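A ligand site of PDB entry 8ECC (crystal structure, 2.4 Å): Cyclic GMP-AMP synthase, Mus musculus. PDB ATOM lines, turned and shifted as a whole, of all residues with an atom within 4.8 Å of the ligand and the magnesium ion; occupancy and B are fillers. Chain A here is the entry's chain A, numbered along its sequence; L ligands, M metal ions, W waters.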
ATOM      1  N   GLY A  55      22.992 -14.094   4.220  1.00  0.00           N
ATOM      2  CA  GLY A  55      22.077 -13.754   5.298  1.00  0.00           C
ATOM      3  C   GLY A  55      21.413 -14.931   5.973  1.00  0.00           C
ATOM      4  O   GLY A  55      21.688 -16.102   5.657  1.00  0.00           O
ATOM      5  N   SER A  56      20.494 -14.606   6.880  1.00  0.00           N
ATOM      6  CA  SER A  56      19.975 -15.541   7.852  1.00  0.00           C
ATOM      7  C   SER A  56      19.327 -16.753   7.219  1.00  0.00           C
ATOM      8  O   SER A  56      19.557 -17.860   7.679  1.00  0.00           O
ATOM      9  CB  SER A  56      19.011 -14.848   8.831  1.00  0.00           C
ATOM     10  OG  SER A  56      17.903 -14.268   8.138  1.00  0.00           O
ATOM     11  N   TYR A  57      18.509 -16.555   6.181  1.00  0.00           N
ATOM     12  CA  TYR A  57      17.725 -17.650   5.538  1.00  0.00           C
ATOM     13  C   TYR A  57      18.670 -18.742   5.039  1.00  0.00           C
ATOM     14  O   TYR A  57      18.377 -19.923   5.247  1.00  0.00           O
ATOM     15  CB  TYR A  57      16.833 -17.155   4.396  1.00  0.00           C
ATOM     16  CG  TYR A  57      16.179 -18.269   3.614  1.00  0.00           C
ATOM     17  CD1 TYR A  57      15.013 -18.881   4.040  1.00  0.00           C
ATOM     18  CD2 TYR A  57      16.744 -18.728   2.429  1.00  0.00           C
ATOM     19  CE1 TYR A  57      14.419 -19.899   3.316  1.00  0.00           C
ATOM     20  CE2 TYR A  57      16.160 -19.746   1.694  1.00  0.00           C
ATOM     21  CZ  TYR A  57      14.999 -20.342   2.135  1.00  0.00           C
ATOM     22  OH  TYR A  57      14.410 -21.341   1.417  1.00  0.00           O
ATOM     23  N   GLU A  59      21.858 -19.123   6.016  1.00  0.00           N
ATOM     24  CA  GLU A  59      22.624 -19.628   7.165  1.00  0.00           C
ATOM     25  C   GLU A  59      21.805 -20.551   8.087  1.00  0.00           C
ATOM     26  O   GLU A  59      22.350 -21.166   9.008  1.00  0.00           O
ATOM     27  CB  GLU A  59      23.151 -18.453   7.974  1.00  0.00           C
ATOM     28  CG  GLU A  59      24.158 -17.608   7.218  1.00  0.00           C
ATOM     29  CD  GLU A  59      24.402 -16.235   7.832  1.00  0.00           C
ATOM     30  OE1 GLU A  59      23.627 -15.780   8.704  1.00  0.00           O
ATOM     31  OE2 GLU A  59      25.381 -15.585   7.416  1.00  0.00           O
ATOM     32  N   LYS A  62      17.237 -17.880  10.166  1.00  0.00           N
ATOM     33  CA  LYS A  62      16.046 -17.070   9.962  1.00  0.00           C
ATOM     34  C   LYS A  62      14.982 -17.623  10.883  1.00  0.00           C
ATOM     35  O   LYS A  62      14.797 -18.833  10.969  1.00  0.00           O
ATOM     36  CB  LYS A  62      15.582 -17.159   8.523  1.00  0.00           C
ATOM     37  CG  LYS A  62      14.387 -16.291   8.190  1.00  0.00           C
ATOM     38  CD  LYS A  62      14.800 -14.831   8.060  1.00  0.00           C
ATOM     39  CE  LYS A  62      13.579 -13.941   7.868  1.00  0.00           C
ATOM     40  NZ  LYS A  62      12.803 -13.709   9.114  1.00  0.00           N
ATOM     41  N   GLU A  68      12.290 -12.637   4.666  1.00  0.00           N
ATOM     42  CA  GLU A  68      13.390 -11.747   4.349  1.00  0.00           C
ATOM     43  C   GLU A  68      14.571 -12.559   3.804  1.00  0.00           C
ATOM     44  O   GLU A  68      15.086 -13.462   4.478  1.00  0.00           O
ATOM     45  CB  GLU A  68      13.797 -10.901   5.564  1.00  0.00           C
ATOM     46  CG  GLU A  68      14.503  -9.577   5.242  1.00  0.00           C
ATOM     47  CD  GLU A  68      16.004  -9.714   5.002  1.00  0.00           C
ATOM     48  OE1 GLU A  68      16.604 -10.737   5.403  1.00  0.00           O
ATOM     49  OE2 GLU A  68      16.596  -8.764   4.440  1.00  0.00           O
ATOM     50  N   PHE A  69      14.988 -12.224   2.581  1.00  0.00           N
ATOM     51  CA  PHE A  69      16.030 -12.920   1.840  1.00  0.00           C
ATOM     52  C   PHE A  69      17.065 -11.890   1.396  1.00  0.00           C
ATOM     53  O   PHE A  69      16.704 -10.787   1.007  1.00  0.00           O
ATOM     54  CB  PHE A  69      15.453 -13.616   0.604  1.00  0.00           C
ATOM     55  CG  PHE A  69      14.432 -14.680   0.925  1.00  0.00           C
ATOM     56  CD1 PHE A  69      13.139 -14.334   1.287  1.00  0.00           C
ATOM     57  CD2 PHE A  69      14.772 -16.023   0.852  1.00  0.00           C
ATOM     58  CE1 PHE A  69      12.192 -15.303   1.582  1.00  0.00           C
ATOM     59  CE2 PHE A  69      13.835 -16.998   1.156  1.00  0.00           C
ATOM     60  CZ  PHE A  69      12.544 -16.643   1.520  1.00  0.00           C
ATOM     61  N   ASP A  70      18.344 -12.246   1.467  1.00  0.00           N
ATOM     62  CA  ASP A  70      19.417 -11.358   1.067  1.00  0.00           C
ATOM     63  C   ASP A  70      20.224 -12.027  -0.031  1.00  0.00           C
ATOM     64  O   ASP A  70      20.603 -13.193   0.101  1.00  0.00           O
ATOM     65  CB  ASP A  70      20.293 -11.018   2.277  1.00  0.00           C
ATOM     66  CG  ASP A  70      19.485 -10.452   3.439  1.00  0.00           C
ATOM     67  OD1 ASP A  70      18.971  -9.327   3.316  1.00  0.00           O
ATOM     68  OD2 ASP A  70      19.366 -11.142   4.481  1.00  0.00           O
ATOM     69  N   ASP A 164      16.414  -8.228  -0.385  1.00  0.00           N
ATOM     70  CA  ASP A 164      17.449  -7.231  -0.559  1.00  0.00           C
ATOM     71  C   ASP A 164      18.415  -7.694  -1.629  1.00  0.00           C
ATOM     72  O   ASP A 164      19.164  -8.649  -1.426  1.00  0.00           O
ATOM     73  CB  ASP A 164      18.210  -7.041   0.765  1.00  0.00           C
ATOM     74  CG  ASP A 164      17.382  -6.371   1.842  1.00  0.00           C
ATOM     75  OD1 ASP A 164      16.360  -5.713   1.513  1.00  0.00           O
ATOM     76  OD2 ASP A 164      17.742  -6.495   3.034  1.00  0.00           O
ATOM     77  N   ARG A 221      31.825  -0.089   1.222  1.00  0.00           N
ATOM     78  CA  ARG A 221      32.099  -0.804   2.498  1.00  0.00           C
ATOM     79  C   ARG A 221      32.434  -2.269   2.213  1.00  0.00           C
ATOM     80  O   ARG A 221      31.797  -2.849   1.311  1.00  0.00           O
ATOM     81  CB  ARG A 221      30.901  -0.726   3.449  1.00  0.00           C
ATOM     82  CG  ARG A 221      31.173  -1.319   4.831  1.00  0.00           C
ATOM     83  CD  ARG A 221      30.025  -1.258   5.830  1.00  0.00           C
ATOM     84  NE  ARG A 221      28.674  -1.495   5.301  1.00  0.00           N
ATOM     85  CZ  ARG A 221      28.186  -2.674   4.927  1.00  0.00           C
ATOM     86  NH1 ARG A 221      28.952  -3.755   4.950  1.00  0.00           N
ATOM     87  NH2 ARG A 221      26.942  -2.763   4.492  1.00  0.00           N
ATOM     88  N   SER A 225      29.932 -11.417   3.909  1.00  0.00           N
ATOM     89  CA  SER A 225      28.726 -12.222   4.031  1.00  0.00           C
ATOM     90  C   SER A 225      28.967 -13.650   3.591  1.00  0.00           C
ATOM     91  O   SER A 225      28.351 -14.563   4.122  1.00  0.00           O
ATOM     92  CB  SER A 225      27.608 -11.642   3.192  1.00  0.00           C
ATOM     93  OG  SER A 225      27.224 -10.391   3.717  1.00  0.00           O
ATOM     94  N   GLU A 228      30.941 -15.257   6.462  1.00  0.00           N
ATOM     95  CA  GLU A 228      30.017 -15.442   7.580  1.00  0.00           C
ATOM     96  C   GLU A 228      29.081 -16.629   7.337  1.00  0.00           C
ATOM     97  O   GLU A 228      28.752 -17.374   8.248  1.00  0.00           O
ATOM     98  CB  GLU A 228      29.228 -14.154   7.802  1.00  0.00           C
ATOM     99  CG  GLU A 228      30.085 -12.952   8.184  1.00  0.00           C
ATOM    100  CD  GLU A 228      29.325 -11.636   8.123  1.00  0.00           C
ATOM    101  OE1 GLU A 228      28.080 -11.665   8.048  1.00  0.00           O
ATOM    102  OE2 GLU A 228      29.976 -10.570   8.124  1.00  0.00           O
ATOM    103  N   LYS A 259      18.625 -13.064  18.323  1.00  0.00           N
ATOM    104  CA  LYS A 259      17.999 -12.353  17.221  1.00  0.00           C
ATOM    105  C   LYS A 259      16.566 -11.977  17.538  1.00  0.00           C
ATOM    106  O   LYS A 259      16.135 -10.856  17.269  1.00  0.00           O
ATOM    107  CB  LYS A 259      18.005 -13.190  15.948  1.00  0.00           C
ATOM    108  CG  LYS A 259      19.337 -13.259  15.249  1.00  0.00           C
ATOM    109  CD  LYS A 259      19.387 -14.448  14.304  1.00  0.00           C
ATOM    110  CE  LYS A 259      18.462 -14.304  13.104  1.00  0.00           C
ATOM    111  NZ  LYS A 259      18.820 -13.144  12.257  1.00  0.00           N
ATOM    112  N   GLU A 263      14.716  -8.476  17.753  1.00  0.00           N
ATOM    113  CA  GLU A 263      13.572  -8.256  16.844  1.00  0.00           C
ATOM    114  C   GLU A 263      12.307  -7.817  17.574  1.00  0.00           C
ATOM    115  O   GLU A 263      11.645  -6.868  17.152  1.00  0.00           O
ATOM    116  CB  GLU A 263      13.250  -9.518  16.032  1.00  0.00           C
ATOM    117  CG  GLU A 263      14.020  -9.635  14.725  1.00  0.00           C
ATOM    118  CD  GLU A 263      13.528 -10.780  13.852  1.00  0.00           C
ATOM    119  OE1 GLU A 263      12.298 -11.042  13.826  1.00  0.00           O
ATOM    120  OE2 GLU A 263      14.357 -11.431  13.165  1.00  0.00           O
ATOM    121  N   SER A 277      20.405  -6.795  13.544  1.00  0.00           N
ATOM    122  CA  SER A 277      20.753  -8.185  13.779  1.00  0.00           C
ATOM    123  C   SER A 277      22.242  -8.471  13.622  1.00  0.00           C
ATOM    124  O   SER A 277      22.761  -9.416  14.211  1.00  0.00           O
ATOM    125  CB  SER A 277      19.954  -9.098  12.845  1.00  0.00           C
ATOM    126  OG  SER A 277      20.166  -8.726  11.506  1.00  0.00           O
ATOM    127  N   TYR A 278      22.940  -7.649  12.837  1.00  0.00           N
ATOM    128  CA  TYR A 278      24.395  -7.807  12.602  1.00  0.00           C
ATOM    129  C   TYR A 278      25.161  -7.638  13.919  1.00  0.00           C
ATOM    130  O   TYR A 278      26.202  -8.300  14.092  1.00  0.00           O
ATOM    131  CB  TYR A 278      24.938  -6.834  11.548  1.00  0.00           C
ATOM    132  CG  TYR A 278      26.304  -7.231  11.068  1.00  0.00           C
ATOM    133  CD1 TYR A 278      26.456  -8.399  10.326  1.00  0.00           C
ATOM    134  CD2 TYR A 278      27.455  -6.511  11.379  1.00  0.00           C
ATOM    135  CE1 TYR A 278      27.695  -8.814   9.883  1.00  0.00           C
ATOM    136  CE2 TYR A 278      28.703  -6.931  10.944  1.00  0.00           C
ATOM    137  CZ  TYR A 278      28.827  -8.089  10.195  1.00  0.00           C
ATOM    138  OH  TYR A 278      30.021  -8.550   9.728  1.00  0.00           O
ATOM    139  N   LYS A 281      24.957 -10.911  15.661  1.00  0.00           N
ATOM    140  CA  LYS A 281      25.754 -11.866  14.898  1.00  0.00           C
ATOM    141  C   LYS A 281      27.249 -11.686  15.183  1.00  0.00           C
ATOM    142  O   LYS A 281      27.984 -12.649  15.353  1.00  0.00           O
ATOM    143  CB  LYS A 281      25.486 -11.705  13.405  1.00  0.00           C
ATOM    144  CG  LYS A 281      25.954 -12.862  12.543  1.00  0.00           C
ATOM    145  CD  LYS A 281      25.885 -12.503  11.065  1.00  0.00           C
ATOM    146  CE  LYS A 281      25.854 -13.748  10.207  1.00  0.00           C
ATOM    147  NZ  LYS A 281      26.015 -13.459   8.752  1.00  0.00           N
ATOM    148  N   HIS A 324      34.056  -5.052  14.817  1.00  0.00           N
ATOM    149  CA  HIS A 324      33.774  -5.824  13.633  1.00  0.00           C
ATOM    150  C   HIS A 324      34.690  -7.050  13.678  1.00  0.00           C
ATOM    151  O   HIS A 324      35.876  -6.939  13.943  1.00  0.00           O
ATOM    152  CB  HIS A 324      34.035  -5.003  12.369  1.00  0.00           C
ATOM    153  CG  HIS A 324      33.384  -5.549  11.133  1.00  0.00           C
ATOM    154  ND1 HIS A 324      33.799  -6.696  10.513  1.00  0.00           N
ATOM    155  CD2 HIS A 324      32.336  -5.085  10.407  1.00  0.00           C
ATOM    156  CE1 HIS A 324      33.047  -6.921   9.460  1.00  0.00           C
ATOM    157  NE2 HIS A 324      32.149  -5.967   9.370  1.00  0.00           N
HETATM  158  P1  LIG L   1      17.969 -11.132   9.431  1.00  0.00           P
HETATM  159  O1  LIG L   1      17.228 -12.385   9.877  1.00  0.00           O
HETATM  160  O2  LIG L   1      17.719 -10.794   7.978  1.00  0.00           O
HETATM  161  O3  LIG L   1      17.739  -9.953  10.363  1.00  0.00           O
HETATM  162  P2  LIG L   1      20.693 -11.343   8.429  1.00  0.00           P
HETATM  163  O4  LIG L   1      21.974 -11.897   8.975  1.00  0.00           O
HETATM  164  O5  LIG L   1      20.158 -11.861   7.129  1.00  0.00           O
HETATM  165  O6  LIG L   1      19.544 -11.471   9.530  1.00  0.00           O
HETATM  166  P3  LIG L   1      20.358  -8.626   7.288  1.00  0.00           P
HETATM  167  O7  LIG L   1      20.074  -7.377   8.062  1.00  0.00           O
HETATM  168  O8  LIG L   1      19.280  -9.201   6.426  1.00  0.00           O
HETATM  169  O9  LIG L   1      20.821  -9.750   8.335  1.00  0.00           O
HETATM  170  O10 LIG L   1      21.688  -8.422   6.426  1.00  0.00           O
HETATM  171  C1  LIG L   1      22.139  -9.485   5.549  1.00  0.00           C
HETATM  172  C2  LIG L   1      23.635  -9.658   5.673  1.00  0.00           C
HETATM  173  O11 LIG L   1      24.300  -8.411   5.360  1.00  0.00           O
HETATM  174  C3  LIG L   1      24.180 -10.037   7.054  1.00  0.00           C
HETATM  175  O12 LIG L   1      24.113 -11.432   7.297  1.00  0.00           O
HETATM  176  C4  LIG L   1      25.617  -9.541   6.960  1.00  0.00           C
HETATM  177  O13 LIG L   1      26.471 -10.474   6.329  1.00  0.00           O
HETATM  178  C5  LIG L   1      25.477  -8.266   6.122  1.00  0.00           C
HETATM  179  N1  LIG L   1      25.365  -7.037   6.913  1.00  0.00           N
HETATM  180  C6  LIG L   1      24.219  -6.434   7.399  1.00  0.00           C
HETATM  181  N2  LIG L   1      24.480  -5.325   8.053  1.00  0.00           N
HETATM  182  C7  LIG L   1      25.855  -5.200   8.001  1.00  0.00           C
HETATM  183  C8  LIG L   1      26.754  -4.232   8.525  1.00  0.00           C
HETATM  184  N3  LIG L   1      26.361  -3.178   9.223  1.00  0.00           N
HETATM  185  N4  LIG L   1      28.077  -4.415   8.282  1.00  0.00           N
HETATM  186  C9  LIG L   1      28.465  -5.490   7.588  1.00  0.00           C
HETATM  187  N5  LIG L   1      27.721  -6.453   7.045  1.00  0.00           N
HETATM  188  C10 LIG L   1      26.415  -6.247   7.305  1.00  0.00           C
HETATM  189 MG    MG M   1      17.676 -12.363   6.219  1.00  0.00          MG
HETATM  190  O   HOH W   1      15.234 -13.622  11.018  1.00  0.00           O
HETATM  191  O   HOH W   2      18.694 -14.157   3.707  1.00  0.00           O
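O13 of the ligand lies within hydrogen-bond range of OE1 of Glu 228 (2.6 Å). N of Ser 56 lies within hydrogen-bond range of O5 of the ligand (2.8 Å). The side-chain hydroxyl (OG) of Ser 56 lies within hydrogen-bond range of an oxygen (O1) of the ligand, 2.7 Å away. The side-chain carboxylate (OD2) of Asp 70 sits close to an oxygen (O8) of the ligand. OG of Ser 225 is in hydrogen-bond range of O13 of the ligand (2.7 Å). O3 of the ligand sits at hydrogen-bond distance from OG of Ser 277 (2.9 Å). An oxygen (O1) of the ligand is in salt-bridge range of the side-chain amino group (NZ) of Lys 259. An oxygen (O12) of the ligand is in hydrogen-bond range of the side-chain amino group (NZ) of Lys 281, at 3.1 Å.
The side-chain carboxylate (OE2) of Glu 68 lies close to the side-chain carboxylate (OD1) of Asp 70. The side-chain carboxylate (OE1) of Glu 228 lies within salt-bridge range of the side-chain amino group (NZ) of Lys 281, 2.8 Å away. OE2 of Glu 228 lies within hydrogen-bond range of OH of Tyr 278, 2.6 Å away. The backbone carbonyl oxygen (O) of Ser 56 sits at hydrogen-bond distance from the backbone NH (N) of Lys 62 (3.4 Å). The side-chain amino group (NZ) of Lys 281 lies within salt-bridge range of the side-chain carboxylate (OE2) of Glu 59 (2.6 Å). NE2 of His 324 lies within hydrogen-bond range of OH of Tyr 278 (3.4 Å).
CA of Gly 55 touches O5 of the ligand (3.3 Å). Lys 62 touches the ligand. NH1 of Arg 221 touches C9 of the ligand, 3.2 Å away. Tyr 278 touches the ligand. Hydrophobic or aromatic side chains within 4 Å of the ligand: Tyr 278. Within 4 Å of the ligand: Gly 55, Ser 56, Lys 62, Glu 68, Asp 70, Arg 221, Ser 225, Glu 228, Lys 259, Ser 277, Tyr 278 and Lys 281. The nearest printed residue that does not touch the ligand is His 324 (4.1 Å).
The nearest printed residue that does not touch the magnesium ion is Lys 62 (4.2 Å).
The magnesium ion is bound by OE1 of Glu 68 (2.1 Å) and O2 of the ligand (2.4 Å). Slightly farther from the magnesium ion lies O5 of the ligand (2.7 Å). Slightly farther from the magnesium ion lies the side-chain hydroxyl (OG) of Ser 56 (2.7 Å). Slightly farther from the magnesium ion lies the side-chain carboxylate (OD2) of Asp 70 (2.7 Å).
Water W1 lies within hydrogen-bond range of an oxygen (O1) of the ligand (2.6 Å), the side-chain amino group (NZ) of Lys 62 (3.1 Å) and the side-chain carboxylate (OE2) of Glu 263 (3.2 Å). Water W2 lies within hydrogen-bond range of N of Asp 70 (3.0 Å) and N of Tyr 57 (3.5 Å).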
